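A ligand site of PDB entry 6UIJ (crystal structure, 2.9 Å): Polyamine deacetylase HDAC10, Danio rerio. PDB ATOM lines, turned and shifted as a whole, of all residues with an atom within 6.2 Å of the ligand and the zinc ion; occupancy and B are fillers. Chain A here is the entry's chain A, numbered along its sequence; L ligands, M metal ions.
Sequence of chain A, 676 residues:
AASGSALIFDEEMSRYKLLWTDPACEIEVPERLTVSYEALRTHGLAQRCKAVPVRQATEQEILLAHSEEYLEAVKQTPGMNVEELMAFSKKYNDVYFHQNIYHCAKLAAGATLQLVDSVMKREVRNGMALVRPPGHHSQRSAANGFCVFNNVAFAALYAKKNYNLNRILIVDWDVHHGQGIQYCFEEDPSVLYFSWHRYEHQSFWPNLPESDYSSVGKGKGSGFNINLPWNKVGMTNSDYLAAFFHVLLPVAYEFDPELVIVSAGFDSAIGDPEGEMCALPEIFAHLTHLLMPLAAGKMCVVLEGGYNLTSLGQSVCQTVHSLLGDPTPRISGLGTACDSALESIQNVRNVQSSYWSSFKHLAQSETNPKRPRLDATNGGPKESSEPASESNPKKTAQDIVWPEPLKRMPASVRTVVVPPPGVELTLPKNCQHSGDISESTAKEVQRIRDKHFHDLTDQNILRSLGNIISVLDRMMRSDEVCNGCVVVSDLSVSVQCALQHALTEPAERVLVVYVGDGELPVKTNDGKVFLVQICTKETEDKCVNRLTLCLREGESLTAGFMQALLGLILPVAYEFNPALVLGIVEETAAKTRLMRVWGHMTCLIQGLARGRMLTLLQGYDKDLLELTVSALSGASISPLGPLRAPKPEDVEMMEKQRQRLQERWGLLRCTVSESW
OD1 of Asp 94 is in salt-bridge range of N2 of the ligand.
The side-chain carboxylate (OE2) of Glu 274 lies within salt-bridge range of a nitrogen (N1) of the ligand (3.4 Å).
S1 of the ligand sits close to OH of Tyr 307, at 3.4 Å.
A ring nitrogen (NE2) of His 136 sits close to a sulfur (S1) of the ligand (3.3 Å).
A sulfur (S1) of the ligand lies close to a ring nitrogen (NE2) of His 137, at 3.8 Å.
N of Gly 305 sits at hydrogen-bond distance from OD1 of Asp 174 (2.9 Å).
NE2 of His 176 sits close to OE1 of Glu 274, at 3.3 Å.
The backbone carbonyl oxygen (O) of Asp 94 lies within hydrogen-bond range of the backbone NH (N) of Phe 146 (2.9 Å).
NE1 of Trp 205 sits at hydrogen-bond distance from OD1 of Asp 94 (3.0 Å).
N of Gly 145 lies close to O of Asp 94 (3.3 Å).
A ring nitrogen (NE2) of His 136 sits at hydrogen-bond distance from a ring nitrogen (NE2) of His 137 (3.0 Å).
The backbone NH (N) of His 137 is in hydrogen-bond range of the side-chain sulfur (SG) of Cys 147.
SG of Cys 147 is in hydrogen-bond range of O of Gly 145.
Merely in contact with the ligand: Ala 24 (3.3 Å), Gly 145 (3.8 Å), Phe 146 (3.3 Å), Trp 205 (3.4 Å) and Gly 305 (3.9 Å).
Of the 23 residues printed, 13 come within 4 Å of the ligand.
Within 4 Å of the zinc ion: Asp 174, His 176 and Asp 267.
The zinc ion is bound by OD2 of Asp 174 (1.9 Å).
The zinc ion is bound by the side-chain carboxylate (OD2) of Asp 267 (2.0 Å).
S1 of the ligand binds the zinc ion.
The zinc ion is bound by a ring nitrogen (ND1) of His 176 (2.3 Å).
The zinc ion has four donor atoms within binding distance.
Slightly farther from the zinc ion lies OD1 of Asp 174 (2.8 Å).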
ATOM      1  N   PRO A  23      -3.204 -21.290  26.142  1.00  0.00           N
ATOM      2  CA  PRO A  23      -2.724 -21.646  24.790  1.00  0.00           C
ATOM      3  C   PRO A  23      -1.665 -20.686  24.265  1.00  0.00           C
ATOM      4  O   PRO A  23      -0.881 -21.079  23.380  1.00  0.00           O
ATOM      5  CB  PRO A  23      -4.000 -21.600  23.940  1.00  0.00           C
ATOM      6  CG  PRO A  23      -5.129 -21.730  24.920  1.00  0.00           C
ATOM      7  CD  PRO A  23      -4.661 -21.062  26.177  1.00  0.00           C
ATOM      8  N   ALA A  24      -1.578 -19.476  24.815  1.00  0.00           N
ATOM      9  CA  ALA A  24      -0.617 -18.497  24.338  1.00  0.00           C
ATOM     10  C   ALA A  24       0.818 -18.915  24.657  1.00  0.00           C
ATOM     11  O   ALA A  24       1.710 -18.750  23.812  1.00  0.00           O
ATOM     12  CB  ALA A  24      -0.910 -17.123  24.957  1.00  0.00           C
ATOM     13  N   CYS A  25       1.042 -19.465  25.849  1.00  0.00           N
ATOM     14  CA  CYS A  25       2.377 -19.706  26.386  1.00  0.00           C
ATOM     15  C   CYS A  25       2.749 -21.173  26.502  1.00  0.00           C
ATOM     16  O   CYS A  25       3.893 -21.482  26.877  1.00  0.00           O
ATOM     17  CB  CYS A  25       2.545 -19.067  27.778  1.00  0.00           C
ATOM     18  SG  CYS A  25       1.771 -17.483  28.107  1.00  0.00           S
ATOM     19  N   ILE A  27       3.644 -23.256  24.465  1.00  0.00           N
ATOM     20  CA  ILE A  27       4.802 -23.619  23.658  1.00  0.00           C
ATOM     21  C   ILE A  27       6.122 -23.373  24.378  1.00  0.00           C
ATOM     22  O   ILE A  27       7.143 -23.905  23.937  1.00  0.00           O
ATOM     23  CB  ILE A  27       4.784 -22.852  22.316  1.00  0.00           C
ATOM     24  CG1 ILE A  27       5.403 -21.468  22.475  1.00  0.00           C
ATOM     25  CG2 ILE A  27       3.348 -22.708  21.804  1.00  0.00           C
ATOM     26  CD1 ILE A  27       5.599 -20.736  21.174  1.00  0.00           C
ATOM     27  N   ASP A  94       0.719 -12.245  26.840  1.00  0.00           N
ATOM     28  CA  ASP A  94       1.432 -13.450  26.411  1.00  0.00           C
ATOM     29  C   ASP A  94       2.695 -13.697  27.241  1.00  0.00           C
ATOM     30  O   ASP A  94       3.763 -13.993  26.715  1.00  0.00           O
ATOM     31  CB  ASP A  94       1.750 -13.399  24.908  1.00  0.00           C
ATOM     32  CG  ASP A  94       0.491 -13.409  24.047  1.00  0.00           C
ATOM     33  OD1 ASP A  94       0.650 -13.370  22.808  1.00  0.00           O
ATOM     34  OD2 ASP A  94      -0.644 -13.457  24.575  1.00  0.00           O
ATOM     35  N   PRO A 134      13.376 -15.663  27.711  1.00  0.00           N
ATOM     36  CA  PRO A 134      13.971 -14.810  26.678  1.00  0.00           C
ATOM     37  C   PRO A 134      13.975 -13.347  27.082  1.00  0.00           C
ATOM     38  O   PRO A 134      13.585 -13.013  28.208  1.00  0.00           O
ATOM     39  CB  PRO A 134      13.083 -15.058  25.453  1.00  0.00           C
ATOM     40  CG  PRO A 134      12.310 -16.301  25.751  1.00  0.00           C
ATOM     41  CD  PRO A 134      12.139 -16.306  27.235  1.00  0.00           C
ATOM     42  N   HIS A 136      13.964 -10.196  24.266  1.00  0.00           N
ATOM     43  CA  HIS A 136      13.758  -9.080  23.341  1.00  0.00           C
ATOM     44  C   HIS A 136      12.349  -8.492  23.336  1.00  0.00           C
ATOM     45  O   HIS A 136      12.153  -7.420  22.762  1.00  0.00           O
ATOM     46  CB  HIS A 136      14.140  -9.482  21.898  1.00  0.00           C
ATOM     47  CG  HIS A 136      13.347 -10.623  21.345  1.00  0.00           C
ATOM     48  ND1 HIS A 136      13.525 -11.099  20.059  1.00  0.00           N
ATOM     49  CD2 HIS A 136      12.374 -11.393  21.890  1.00  0.00           C
ATOM     50  CE1 HIS A 136      12.699 -12.105  19.846  1.00  0.00           C
ATOM     51  NE2 HIS A 136      11.997 -12.305  20.934  1.00  0.00           N
ATOM     52  N   HIS A 137      11.373  -9.136  23.968  1.00  0.00           N
ATOM     53  CA  HIS A 137      10.026  -8.594  24.013  1.00  0.00           C
ATOM     54  C   HIS A 137       9.756  -7.768  25.269  1.00  0.00           C
ATOM     55  O   HIS A 137       8.742  -7.064  25.312  1.00  0.00           O
ATOM     56  CB  HIS A 137       8.993  -9.705  23.915  1.00  0.00           C
ATOM     57  CG  HIS A 137       9.002 -10.424  22.605  1.00  0.00           C
ATOM     58  ND1 HIS A 137       8.908  -9.780  21.398  1.00  0.00           N
ATOM     59  CD2 HIS A 137       9.092 -11.749  22.323  1.00  0.00           C
ATOM     60  CE1 HIS A 137       8.934 -10.672  20.417  1.00  0.00           C
ATOM     61  NE2 HIS A 137       9.058 -11.870  20.948  1.00  0.00           N
ATOM     62  N   GLY A 145       5.502 -11.316  26.041  1.00  0.00           N
ATOM     63  CA  GLY A 145       5.919 -12.376  25.134  1.00  0.00           C
ATOM     64  C   GLY A 145       7.021 -13.258  25.695  1.00  0.00           C
ATOM     65  O   GLY A 145       8.144 -13.275  25.175  1.00  0.00           O
ATOM     66  N   PHE A 146       6.697 -13.974  26.787  1.00  0.00           N
ATOM     67  CA  PHE A 146       7.563 -14.959  27.440  1.00  0.00           C
ATOM     68  C   PHE A 146       8.786 -14.314  28.106  1.00  0.00           C
ATOM     69  O   PHE A 146       9.530 -15.005  28.800  1.00  0.00           O
ATOM     70  CB  PHE A 146       8.049 -16.036  26.447  1.00  0.00           C
ATOM     71  CG  PHE A 146       6.941 -16.723  25.671  1.00  0.00           C
ATOM     72  CD1 PHE A 146       5.605 -16.605  26.034  1.00  0.00           C
ATOM     73  CD2 PHE A 146       7.245 -17.494  24.557  1.00  0.00           C
ATOM     74  CE1 PHE A 146       4.598 -17.233  25.306  1.00  0.00           C
ATOM     75  CE2 PHE A 146       6.251 -18.143  23.824  1.00  0.00           C
ATOM     76  CZ  PHE A 146       4.931 -18.001  24.195  1.00  0.00           C
ATOM     77  N   CYS A 147       8.995 -13.006  27.930  1.00  0.00           N
ATOM     78  CA  CYS A 147      10.159 -12.311  28.469  1.00  0.00           C
ATOM     79  C   CYS A 147       9.806 -11.552  29.735  1.00  0.00           C
ATOM     80  O   CYS A 147       8.664 -11.126  29.937  1.00  0.00           O
ATOM     81  CB  CYS A 147      10.737 -11.332  27.443  1.00  0.00           C
ATOM     82  SG  CYS A 147      11.000 -12.030  25.805  1.00  0.00           S
ATOM     83  N   ASP A 174      15.648 -13.918  15.703  1.00  0.00           N
ATOM     84  CA  ASP A 174      14.379 -14.503  16.103  1.00  0.00           C
ATOM     85  C   ASP A 174      13.286 -14.079  15.116  1.00  0.00           C
ATOM     86  O   ASP A 174      13.398 -13.053  14.433  1.00  0.00           O
ATOM     87  CB  ASP A 174      14.034 -14.056  17.518  1.00  0.00           C
ATOM     88  CG  ASP A 174      12.942 -14.893  18.142  1.00  0.00           C
ATOM     89  OD1 ASP A 174      13.258 -15.682  19.047  1.00  0.00           O
ATOM     90  OD2 ASP A 174      11.770 -14.746  17.743  1.00  0.00           O
ATOM     91  N   VAL A 175      12.224 -14.880  15.016  1.00  0.00           N
ATOM     92  CA  VAL A 175      11.172 -14.621  14.039  1.00  0.00           C
ATOM     93  C   VAL A 175      10.120 -13.653  14.551  1.00  0.00           C
ATOM     94  O   VAL A 175       9.254 -13.225  13.774  1.00  0.00           O
ATOM     95  CB  VAL A 175      10.528 -15.946  13.570  1.00  0.00           C
ATOM     96  CG1 VAL A 175       9.430 -16.380  14.530  1.00  0.00           C
ATOM     97  CG2 VAL A 175       9.993 -15.833  12.144  1.00  0.00           C
ATOM     98  N   HIS A 176      10.160 -13.287  15.823  1.00  0.00           N
ATOM     99  CA  HIS A 176       9.326 -12.214  16.341  1.00  0.00           C
ATOM    100  C   HIS A 176      10.147 -10.944  16.429  1.00  0.00           C
ATOM    101  O   HIS A 176      11.377 -10.978  16.537  1.00  0.00           O
ATOM    102  CB  HIS A 176       8.771 -12.551  17.717  1.00  0.00           C
ATOM    103  CG  HIS A 176       7.958 -13.799  17.756  1.00  0.00           C
ATOM    104  ND1 HIS A 176       8.524 -15.056  17.743  1.00  0.00           N
ATOM    105  CD2 HIS A 176       6.620 -13.988  17.856  1.00  0.00           C
ATOM    106  CE1 HIS A 176       7.575 -15.970  17.807  1.00  0.00           C
ATOM    107  NE2 HIS A 176       6.408 -15.348  17.877  1.00  0.00           N
ATOM    108  N   PHE A 204       0.578 -10.491  12.351  1.00  0.00           N
ATOM    109  CA  PHE A 204       1.204 -11.419  13.280  1.00  0.00           C
ATOM    110  C   PHE A 204       1.687 -10.727  14.546  1.00  0.00           C
ATOM    111  O   PHE A 204       2.031  -9.542  14.549  1.00  0.00           O
ATOM    112  CB  PHE A 204       2.386 -12.142  12.633  1.00  0.00           C
ATOM    113  CG  PHE A 204       2.907 -13.296  13.457  1.00  0.00           C
ATOM    114  CD1 PHE A 204       2.099 -14.395  13.711  1.00  0.00           C
ATOM    115  CD2 PHE A 204       4.188 -13.265  13.985  1.00  0.00           C
ATOM    116  CE1 PHE A 204       2.551 -15.447  14.468  1.00  0.00           C
ATOM    117  CE2 PHE A 204       4.649 -14.315  14.757  1.00  0.00           C
ATOM    118  CZ  PHE A 204       3.831 -15.409  15.002  1.00  0.00           C
ATOM    119  N   TRP A 205       1.726 -11.505  15.634  1.00  0.00           N
ATOM    120  CA  TRP A 205       2.132 -11.013  16.937  1.00  0.00           C
ATOM    121  C   TRP A 205       3.561 -10.461  16.879  1.00  0.00           C
ATOM    122  O   TRP A 205       4.455 -11.108  16.312  1.00  0.00           O
ATOM    123  CB  TRP A 205       2.027 -12.140  17.972  1.00  0.00           C
ATOM    124  CG  TRP A 205       2.133 -11.652  19.365  1.00  0.00           C
ATOM    125  CD1 TRP A 205       1.097 -11.308  20.190  1.00  0.00           C
ATOM    126  CD2 TRP A 205       3.333 -11.428  20.098  1.00  0.00           C
ATOM    127  NE1 TRP A 205       1.588 -10.882  21.404  1.00  0.00           N
ATOM    128  CE2 TRP A 205       2.964 -10.942  21.361  1.00  0.00           C
ATOM    129  CE3 TRP A 205       4.699 -11.581  19.810  1.00  0.00           C
ATOM    130  CZ2 TRP A 205       3.900 -10.615  22.345  1.00  0.00           C
ATOM    131  CZ3 TRP A 205       5.626 -11.250  20.772  1.00  0.00           C
ATOM    132  CH2 TRP A 205       5.219 -10.783  22.032  1.00  0.00           C
ATOM    133  N   GLY A 265      17.182 -16.487  18.120  1.00  0.00           N
ATOM    134  CA  GLY A 265      15.899 -17.163  18.181  1.00  0.00           C
ATOM    135  C   GLY A 265      15.820 -18.169  17.048  1.00  0.00           C
ATOM    136  O   GLY A 265      16.085 -17.828  15.890  1.00  0.00           O
ATOM    137  N   ASP A 267      13.025 -20.088  16.481  1.00  0.00           N
ATOM    138  CA  ASP A 267      11.699 -20.207  15.890  1.00  0.00           C
ATOM    139  C   ASP A 267      11.677 -19.738  14.440  1.00  0.00           C
ATOM    140  O   ASP A 267      10.672 -19.936  13.750  1.00  0.00           O
ATOM    141  CB  ASP A 267      10.679 -19.445  16.740  1.00  0.00           C
ATOM    142  CG  ASP A 267      11.180 -18.083  17.167  1.00  0.00           C
ATOM    143  OD1 ASP A 267      12.222 -17.625  16.635  1.00  0.00           O
ATOM    144  OD2 ASP A 267      10.539 -17.452  18.032  1.00  0.00           O
ATOM    145  N   GLU A 274       5.497 -21.623  15.552  1.00  0.00           N
ATOM    146  CA  GLU A 274       5.224 -20.208  15.695  1.00  0.00           C
ATOM    147  C   GLU A 274       5.797 -19.363  14.561  1.00  0.00           C
ATOM    148  O   GLU A 274       5.217 -18.342  14.199  1.00  0.00           O
ATOM    149  CB  GLU A 274       5.777 -19.710  17.038  1.00  0.00           C
ATOM    150  CG  GLU A 274       5.458 -18.283  17.369  1.00  0.00           C
ATOM    151  CD  GLU A 274       4.158 -18.119  18.109  1.00  0.00           C
ATOM    152  OE1 GLU A 274       3.610 -16.996  18.108  1.00  0.00           O
ATOM    153  OE2 GLU A 274       3.689 -19.131  18.684  1.00  0.00           O
ATOM    154  N   GLU A 304      16.948 -16.887  22.472  1.00  0.00           N
ATOM    155  CA  GLU A 304      15.652 -16.248  22.616  1.00  0.00           C
ATOM    156  C   GLU A 304      14.587 -17.316  22.464  1.00  0.00           C
ATOM    157  O   GLU A 304      14.331 -18.082  23.414  1.00  0.00           O
ATOM    158  CB  GLU A 304      15.499 -15.101  21.609  1.00  0.00           C
ATOM    159  CG  GLU A 304      16.479 -13.935  21.785  1.00  0.00           C
ATOM    160  CD  GLU A 304      16.040 -12.961  22.872  1.00  0.00           C
ATOM    161  OE1 GLU A 304      15.056 -13.266  23.580  1.00  0.00           O
ATOM    162  OE2 GLU A 304      16.679 -11.888  23.032  1.00  0.00           O
ATOM    163  N   GLY A 305      13.953 -17.437  21.289  1.00  0.00           N
ATOM    164  CA  GLY A 305      12.924 -18.420  21.051  1.00  0.00           C
ATOM    165  C   GLY A 305      13.430 -19.607  20.242  1.00  0.00           C
ATOM    166  O   GLY A 305      14.612 -19.721  19.902  1.00  0.00           O
ATOM    167  N   GLY A 306      12.477 -20.493  19.899  1.00  0.00           N
ATOM    168  CA  GLY A 306      12.730 -21.780  19.266  1.00  0.00           C
ATOM    169  C   GLY A 306      11.953 -22.850  20.003  1.00  0.00           C
ATOM    170  O   GLY A 306      12.298 -23.203  21.126  1.00  0.00           O
ATOM    171  N   TYR A 307      10.883 -23.373  19.386  1.00  0.00           N
ATOM    172  CA  TYR A 307       9.870 -24.107  20.139  1.00  0.00           C
ATOM    173  C   TYR A 307       9.562 -25.488  19.593  1.00  0.00           C
ATOM    174  O   TYR A 307       8.708 -26.184  20.173  1.00  0.00           O
ATOM    175  CB  TYR A 307       8.584 -23.271  20.219  1.00  0.00           C
ATOM    176  CG  TYR A 307       8.841 -21.922  20.819  1.00  0.00           C
ATOM    177  CD1 TYR A 307       8.848 -21.754  22.197  1.00  0.00           C
ATOM    178  CD2 TYR A 307       9.114 -20.825  20.019  1.00  0.00           C
ATOM    179  CE1 TYR A 307       9.093 -20.523  22.759  1.00  0.00           C
ATOM    180  CE2 TYR A 307       9.368 -19.586  20.574  1.00  0.00           C
ATOM    181  CZ  TYR A 307       9.359 -19.442  21.945  1.00  0.00           C
ATOM    182  OH  TYR A 307       9.604 -18.218  22.514  1.00  0.00           O
HETATM  183  C1  LIG L   1       0.673 -17.762  20.838  1.00  0.00           C
HETATM  184  C2  LIG L   1       2.057 -17.094  20.792  1.00  0.00           C
HETATM  185  C3  LIG L   1       2.004 -15.677  21.371  1.00  0.00           C
HETATM  186  C4  LIG L   1       4.323 -15.212  22.006  1.00  0.00           C
HETATM  187  C5  LIG L   1       5.631 -14.622  21.475  1.00  0.00           C
HETATM  188  C6  LIG L   1       6.790 -15.468  21.904  1.00  0.00           C
HETATM  189  C7  LIG L   1       8.025 -15.113  21.135  1.00  0.00           C
HETATM  190  C8  LIG L   1       9.196 -15.168  22.063  1.00  0.00           C
HETATM  191  N1  LIG L   1       0.481 -18.858  19.884  1.00  0.00           N
HETATM  192  N2  LIG L   1       3.244 -14.972  21.014  1.00  0.00           N
HETATM  193  S1  LIG L   1      10.600 -15.329  20.997  1.00  0.00           S
HETATM  194 ZN    ZN M   1      10.496 -15.636  18.865  1.00  0.00          ZN
